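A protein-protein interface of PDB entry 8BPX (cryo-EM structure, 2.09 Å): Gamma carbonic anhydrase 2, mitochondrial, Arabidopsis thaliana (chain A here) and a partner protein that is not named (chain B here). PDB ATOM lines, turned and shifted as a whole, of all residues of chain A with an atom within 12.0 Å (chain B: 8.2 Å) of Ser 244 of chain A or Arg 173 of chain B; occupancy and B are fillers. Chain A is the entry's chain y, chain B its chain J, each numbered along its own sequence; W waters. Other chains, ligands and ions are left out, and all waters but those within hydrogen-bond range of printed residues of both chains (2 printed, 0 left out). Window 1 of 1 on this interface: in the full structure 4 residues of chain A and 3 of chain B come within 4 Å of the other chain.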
ATOM      1  N   LYS A 238      26.523 -10.573 -18.316  1.00  0.00           N
ATOM      2  CA  LYS A 238      25.535 -11.331 -17.560  1.00  0.00           C
ATOM      3  C   LYS A 238      26.205 -12.455 -16.783  1.00  0.00           C
ATOM      4  O   LYS A 238      27.308 -12.898 -17.115  1.00  0.00           O
ATOM      5  CB  LYS A 238      24.448 -11.906 -18.478  1.00  0.00           C
ATOM      6  CG  LYS A 238      24.934 -12.270 -19.869  1.00  0.00           C
ATOM      7  CD  LYS A 238      23.784 -12.711 -20.763  1.00  0.00           C
ATOM      8  CE  LYS A 238      22.876 -11.548 -21.125  1.00  0.00           C
ATOM      9  NZ  LYS A 238      21.898 -11.923 -22.184  1.00  0.00           N
ATOM     10  N   ASP A 239      25.520 -12.894 -15.707  1.00  0.00           N
ATOM     11  CA  ASP A 239      25.818 -14.154 -15.013  1.00  0.00           C
ATOM     12  C   ASP A 239      24.484 -14.869 -14.809  1.00  0.00           C
ATOM     13  O   ASP A 239      23.887 -14.812 -13.733  1.00  0.00           O
ATOM     14  CB  ASP A 239      26.527 -13.919 -13.684  1.00  0.00           C
ATOM     15  CG  ASP A 239      27.018 -15.207 -13.033  1.00  0.00           C
ATOM     16  OD1 ASP A 239      26.792 -16.303 -13.591  1.00  0.00           O
ATOM     17  OD2 ASP A 239      27.647 -15.120 -11.959  1.00  0.00           O
ATOM     18  N   GLU A 240      24.035 -15.580 -15.843  1.00  0.00           N
ATOM     19  CA  GLU A 240      22.742 -16.248 -15.767  1.00  0.00           C
ATOM     20  C   GLU A 240      22.756 -17.421 -14.798  1.00  0.00           C
ATOM     21  O   GLU A 240      21.709 -17.764 -14.245  1.00  0.00           O
ATOM     22  CB  GLU A 240      22.312 -16.714 -17.156  1.00  0.00           C
ATOM     23  CG  GLU A 240      22.200 -15.591 -18.168  1.00  0.00           C
ATOM     24  CD  GLU A 240      21.176 -15.882 -19.248  1.00  0.00           C
ATOM     25  OE1 GLU A 240      21.528 -15.787 -20.442  1.00  0.00           O
ATOM     26  OE2 GLU A 240      20.021 -16.205 -18.901  1.00  0.00           O
ATOM     27  N   ASP A 241      23.917 -18.034 -14.577  1.00  0.00           N
ATOM     28  CA  ASP A 241      24.003 -19.127 -13.616  1.00  0.00           C
ATOM     29  C   ASP A 241      23.745 -18.642 -12.192  1.00  0.00           C
ATOM     30  O   ASP A 241      22.995 -19.275 -11.437  1.00  0.00           O
ATOM     31  CB  ASP A 241      25.371 -19.792 -13.722  1.00  0.00           C
ATOM     32  CG  ASP A 241      25.449 -21.073 -12.943  1.00  0.00           C
ATOM     33  OD1 ASP A 241      24.425 -21.781 -12.851  1.00  0.00           O
ATOM     34  OD2 ASP A 241      26.535 -21.365 -12.414  1.00  0.00           O
ATOM     35  N   TYR A 242      24.342 -17.512 -11.810  1.00  0.00           N
ATOM     36  CA  TYR A 242      24.075 -16.969 -10.483  1.00  0.00           C
ATOM     37  C   TYR A 242      22.647 -16.460 -10.364  1.00  0.00           C
ATOM     38  O   TYR A 242      22.058 -16.531  -9.282  1.00  0.00           O
ATOM     39  CB  TYR A 242      25.058 -15.853 -10.141  1.00  0.00           C
ATOM     40  CG  TYR A 242      25.196 -15.619  -8.653  1.00  0.00           C
ATOM     41  CD1 TYR A 242      25.899 -16.514  -7.857  1.00  0.00           C
ATOM     42  CD2 TYR A 242      24.614 -14.515  -8.046  1.00  0.00           C
ATOM     43  CE1 TYR A 242      26.030 -16.310  -6.501  1.00  0.00           C
ATOM     44  CE2 TYR A 242      24.738 -14.299  -6.683  1.00  0.00           C
ATOM     45  CZ  TYR A 242      25.448 -15.201  -5.916  1.00  0.00           C
ATOM     46  OH  TYR A 242      25.581 -15.001  -4.564  1.00  0.00           O
ATOM     47  N   ASP A 243      22.080 -15.934 -11.454  1.00  0.00           N
ATOM     48  CA  ASP A 243      20.671 -15.555 -11.435  1.00  0.00           C
ATOM     49  C   ASP A 243      19.780 -16.767 -11.199  1.00  0.00           C
ATOM     50  O   ASP A 243      18.819 -16.698 -10.427  1.00  0.00           O
ATOM     51  CB  ASP A 243      20.290 -14.857 -12.741  1.00  0.00           C
ATOM     52  CG  ASP A 243      20.847 -13.450 -12.834  1.00  0.00           C
ATOM     53  OD1 ASP A 243      21.712 -13.203 -13.696  1.00  0.00           O
ATOM     54  OD2 ASP A 243      20.424 -12.592 -12.035  1.00  0.00           O
ATOM     55  N   SER A 244      20.088 -17.889 -11.856  1.00  0.00           N
ATOM     56  CA  SER A 244      19.321 -19.108 -11.628  1.00  0.00           C
ATOM     57  C   SER A 244      19.468 -19.582 -10.188  1.00  0.00           C
ATOM     58  O   SER A 244      18.506 -20.076  -9.591  1.00  0.00           O
ATOM     59  CB  SER A 244      19.753 -20.198 -12.609  1.00  0.00           C
ATOM     60  OG  SER A 244      20.835 -20.950 -12.098  1.00  0.00           O
ATOM     61  N   MET A 245      20.666 -19.438  -9.612  1.00  0.00           N
ATOM     62  CA  MET A 245      20.816 -19.730  -8.189  1.00  0.00           C
ATOM     63  C   MET A 245      19.929 -18.818  -7.349  1.00  0.00           C
ATOM     64  O   MET A 245      19.285 -19.272  -6.396  1.00  0.00           O
ATOM     65  CB  MET A 245      22.275 -19.597  -7.751  1.00  0.00           C
ATOM     66  CG  MET A 245      22.531 -20.163  -6.355  1.00  0.00           C
ATOM     67  SD  MET A 245      23.983 -19.500  -5.511  1.00  0.00           S
ATOM     68  CE  MET A 245      23.399 -17.872  -5.060  1.00  0.00           C
ATOM     69  N   LEU A 246      19.877 -17.530  -7.692  1.00  0.00           N
ATOM     70  CA  LEU A 246      19.011 -16.592  -6.990  1.00  0.00           C
ATOM     71  C   LEU A 246      17.544 -16.773  -7.355  1.00  0.00           C
ATOM     72  O   LEU A 246      16.676 -16.250  -6.651  1.00  0.00           O
ATOM     73  CB  LEU A 246      19.439 -15.152  -7.288  1.00  0.00           C
ATOM     74  CG  LEU A 246      20.672 -14.601  -6.564  1.00  0.00           C
ATOM     75  CD1 LEU A 246      21.227 -13.377  -7.282  1.00  0.00           C
ATOM     76  CD2 LEU A 246      20.335 -14.268  -5.123  1.00  0.00           C
ATOM     77  N   GLY A 247      17.251 -17.500  -8.428  1.00  0.00           N
ATOM     78  CA  GLY A 247      15.882 -17.653  -8.888  1.00  0.00           C
ATOM     79  C   GLY A 247      15.262 -16.387  -9.441  1.00  0.00           C
ATOM     80  O   GLY A 247      14.081 -16.122  -9.192  1.00  0.00           O
ATOM     81  N   ILE A 248      16.032 -15.596 -10.185  1.00  0.00           N
ATOM     82  CA  ILE A 248      15.540 -14.373 -10.803  1.00  0.00           C
ATOM     83  C   ILE A 248      15.937 -14.380 -12.270  1.00  0.00           C
ATOM     84  O   ILE A 248      16.840 -15.104 -12.693  1.00  0.00           O
ATOM     85  CB  ILE A 248      16.078 -13.097 -10.119  1.00  0.00           C
ATOM     86  CG1 ILE A 248      17.587 -12.972 -10.350  1.00  0.00           C
ATOM     87  CG2 ILE A 248      15.741 -13.091  -8.638  1.00  0.00           C
ATOM     88  CD1 ILE A 248      18.123 -11.575 -10.150  1.00  0.00           C
ATOM     89  N   THR A 249      15.253 -13.548 -13.049  1.00  0.00           N
ATOM     90  CA  THR A 249      15.529 -13.417 -14.475  1.00  0.00           C
ATOM     91  C   THR A 249      15.630 -11.937 -14.809  1.00  0.00           C
ATOM     92  O   THR A 249      14.626 -11.217 -14.776  1.00  0.00           O
ATOM     93  CB  THR A 249      14.452 -14.096 -15.315  1.00  0.00           C
ATOM     94  OG1 THR A 249      14.484 -15.507 -15.076  1.00  0.00           O
ATOM     95  CG2 THR A 249      14.699 -13.836 -16.790  1.00  0.00           C
ATOM     96  N   ARG A 250      16.839 -11.489 -15.123  1.00  0.00           N
ATOM     97  CA  ARG A 250      17.069 -10.097 -15.474  1.00  0.00           C
ATOM     98  C   ARG A 250      16.599  -9.848 -16.899  1.00  0.00           C
ATOM     99  O   ARG A 250      16.964 -10.583 -17.820  1.00  0.00           O
ATOM    100  CB  ARG A 250      18.549  -9.755 -15.321  1.00  0.00           C
ATOM    101  CG  ARG A 250      19.125 -10.199 -13.986  1.00  0.00           C
ATOM    102  CD  ARG A 250      20.392  -9.455 -13.642  1.00  0.00           C
ATOM    103  NE  ARG A 250      21.009  -9.974 -12.428  1.00  0.00           N
ATOM    104  CZ  ARG A 250      20.829  -9.457 -11.222  1.00  0.00           C
ATOM    105  NH1 ARG A 250      20.036  -8.417 -11.028  1.00  0.00           N
ATOM    106  NH2 ARG A 250      21.461  -9.996 -10.183  1.00  0.00           N
ATOM    107  N   GLU A 251      15.782  -8.818 -17.075  1.00  0.00           N
ATOM    108  CA  GLU A 251      15.232  -8.470 -18.375  1.00  0.00           C
ATOM    109  C   GLU A 251      15.846  -7.166 -18.861  1.00  0.00           C
ATOM    110  O   GLU A 251      16.089  -6.250 -18.070  1.00  0.00           O
ATOM    111  CB  GLU A 251      13.706  -8.347 -18.308  1.00  0.00           C
ATOM    112  CG  GLU A 251      12.896  -9.663 -18.182  1.00  0.00           C
ATOM    113  CD  GLU A 251      13.231 -10.769 -19.195  1.00  0.00           C
ATOM    114  OE1 GLU A 251      14.349 -10.837 -19.747  1.00  0.00           O
ATOM    115  OE2 GLU A 251      12.334 -11.605 -19.439  1.00  0.00           O
ATOM    116  N   ILE B 167      25.312 -25.318  -1.009  1.00  0.00           N
ATOM    117  CA  ILE B 167      24.394 -24.330  -1.575  1.00  0.00           C
ATOM    118  C   ILE B 167      24.925 -23.794  -2.905  1.00  0.00           C
ATOM    119  O   ILE B 167      24.223 -23.817  -3.920  1.00  0.00           O
ATOM    120  CB  ILE B 167      24.123 -23.191  -0.578  1.00  0.00           C
ATOM    121  CG1 ILE B 167      23.320 -23.701   0.621  1.00  0.00           C
ATOM    122  CG2 ILE B 167      23.390 -22.054  -1.279  1.00  0.00           C
ATOM    123  CD1 ILE B 167      22.144 -24.575   0.256  1.00  0.00           C
ATOM    124  N   THR B 170      24.859 -26.405  -6.052  1.00  0.00           N
ATOM    125  CA  THR B 170      23.669 -27.109  -6.513  1.00  0.00           C
ATOM    126  C   THR B 170      22.381 -26.292  -6.512  1.00  0.00           C
ATOM    127  O   THR B 170      21.429 -26.698  -7.183  1.00  0.00           O
ATOM    128  CB  THR B 170      23.431 -28.377  -5.674  1.00  0.00           C
ATOM    129  OG1 THR B 170      23.173 -28.016  -4.314  1.00  0.00           O
ATOM    130  CG2 THR B 170      24.648 -29.296  -5.732  1.00  0.00           C
ATOM    131  N   MET B 171      22.320 -25.169  -5.800  1.00  0.00           N
ATOM    132  CA  MET B 171      21.056 -24.458  -5.627  1.00  0.00           C
ATOM    133  C   MET B 171      20.543 -23.883  -6.943  1.00  0.00           C
ATOM    134  O   MET B 171      21.266 -23.187  -7.659  1.00  0.00           O
ATOM    135  CB  MET B 171      21.218 -23.337  -4.601  1.00  0.00           C
ATOM    136  CG  MET B 171      19.946 -22.558  -4.295  1.00  0.00           C
ATOM    137  SD  MET B 171      18.446 -23.557  -4.340  1.00  0.00           S
ATOM    138  CE  MET B 171      18.079 -23.664  -2.593  1.00  0.00           C
ATOM    139  N   HIS B 172      19.280 -24.176  -7.249  1.00  0.00           N
ATOM    140  CA  HIS B 172      18.525 -23.537  -8.327  1.00  0.00           C
ATOM    141  C   HIS B 172      17.190 -23.134  -7.706  1.00  0.00           C
ATOM    142  O   HIS B 172      16.273 -23.953  -7.615  1.00  0.00           O
ATOM    143  CB  HIS B 172      18.336 -24.466  -9.524  1.00  0.00           C
ATOM    144  CG  HIS B 172      19.569 -24.656 -10.349  1.00  0.00           C
ATOM    145  ND1 HIS B 172      20.613 -25.464  -9.954  1.00  0.00           N
ATOM    146  CD2 HIS B 172      19.925 -24.144 -11.550  1.00  0.00           C
ATOM    147  CE1 HIS B 172      21.559 -25.439 -10.874  1.00  0.00           C
ATOM    148  NE2 HIS B 172      21.167 -24.644 -11.853  1.00  0.00           N
ATOM    149  N   ARG B 173      17.090 -21.884  -7.260  1.00  0.00           N
ATOM    150  CA  ARG B 173      15.894 -21.434  -6.560  1.00  0.00           C
ATOM    151  C   ARG B 173      14.738 -21.269  -7.540  1.00  0.00           C
ATOM    152  O   ARG B 173      14.893 -20.665  -8.605  1.00  0.00           O
ATOM    153  CB  ARG B 173      16.170 -20.119  -5.830  1.00  0.00           C
ATOM    154  CG  ARG B 173      15.130 -19.752  -4.780  1.00  0.00           C
ATOM    155  CD  ARG B 173      15.556 -18.533  -3.975  1.00  0.00           C
ATOM    156  NE  ARG B 173      14.794 -18.395  -2.740  1.00  0.00           N
ATOM    157  CZ  ARG B 173      15.200 -17.707  -1.682  1.00  0.00           C
ATOM    158  NH1 ARG B 173      16.363 -17.077  -1.671  1.00  0.00           N
ATOM    159  NH2 ARG B 173      14.421 -17.653  -0.605  1.00  0.00           N
ATOM    160  N   THR B 174      13.581 -21.809  -7.181  1.00  0.00           N
ATOM    161  CA  THR B 174      12.410 -21.732  -8.047  1.00  0.00           C
ATOM    162  C   THR B 174      11.885 -20.303  -8.135  1.00  0.00           C
ATOM    163  O   THR B 174      11.895 -19.696  -9.207  1.00  0.00           O
ATOM    164  CB  THR B 174      11.284 -22.658  -7.560  1.00  0.00           C
ATOM    165  OG1 THR B 174      11.787 -23.993  -7.428  1.00  0.00           O
ATOM    166  CG2 THR B 174      10.132 -22.653  -8.551  1.00  0.00           C
HETATM  167  O   HOH W   1      16.279 -21.155 -10.641  1.00  0.00           O
HETATM  168  O   HOH W   2      17.190 -14.646  -3.818  1.00  0.00           O
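Ser 244 of chain A touches His 172 of chain B. Met 245 of chain A touches Met 171 of chain B. Arg 173 of chain B touches Met 245 of chain A. Arg 173 of chain B touches Leu 246 of chain A (CD to O, 3.7 Å). CA of Gly 247 of chain A touches O of Arg 173 of chain B, at 3.2 Å.
N of Arg 173 of chain B is in hydrogen-bond range of O of Ser 244 of chain A, 3.3 Å away.
Of chain B, only His 172 (3.4 Å) and Arg 173 (3.3 Å) come within 4 Å of Ser 244 of chain A. Printed residues of chain B within 4 Å of Met 245 of chain A: Met 171 (3.5 Å) and Arg 173 (3.3 Å). Of the printed residues of chain B, Leu 246 of chain A touches Arg 173. Of the printed residues of chain B, Gly 247 of chain A touches Arg 173 (3.2 Å). Of chain A, only Met 245 (3.5 Å) comes within 4 Å of Met 171 of chain B. Of chain A, only Ser 244 (3.4 Å) comes within 4 Å of His 172 of chain B. Of chain A, only Ser 244, Met 245, Leu 246 and Gly 247 come within 4 Å of Arg 173 of chain B. No residue of chain A comes within 4 Å of Thr 174 of chain B. The nearest printed residue of chain B that does not touch Leu 246 of chain A is Met 171 of chain B (5.8 Å).
Water W1 bridges the backbone carbonyl oxygen (O) of Arg 173 of chain B (2.5 Å) and the backbone carbonyl oxygen (O) of Ser 244 of chain A (2.7 Å). Water W2 lies within hydrogen-bond range of the backbone carbonyl oxygen (O) of Leu 246 of chain A (3.3 Å) and the guanidinium group (NH1) of Arg 173 of chain B (3.3 Å).
The backbone NH (N) of Arg 173 of chain B sits at hydrogen-bond distance from the side-chain sulfur (SD) of Met 171 of chain B (3.6 Å). O of Asp 241 of chain A lies within hydrogen-bond range of OG of Ser 244 of chain A. O of Thr 170 of chain B sits at hydrogen-bond distance from ND1 of His 172 of chain B.
Hydrophobic or aromatic side chains of chain A that line the printed part of chain B: Met 245. Along chain A the printed residues that touch a printed residue of chain B span positions 244 to 247. Among the printed residues, 6 pairs touch across the chains. Among the printed residues, no Asp or Glu carboxylate lies within 4 Å of a Lys or Arg side-chain nitrogen of the other chain.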
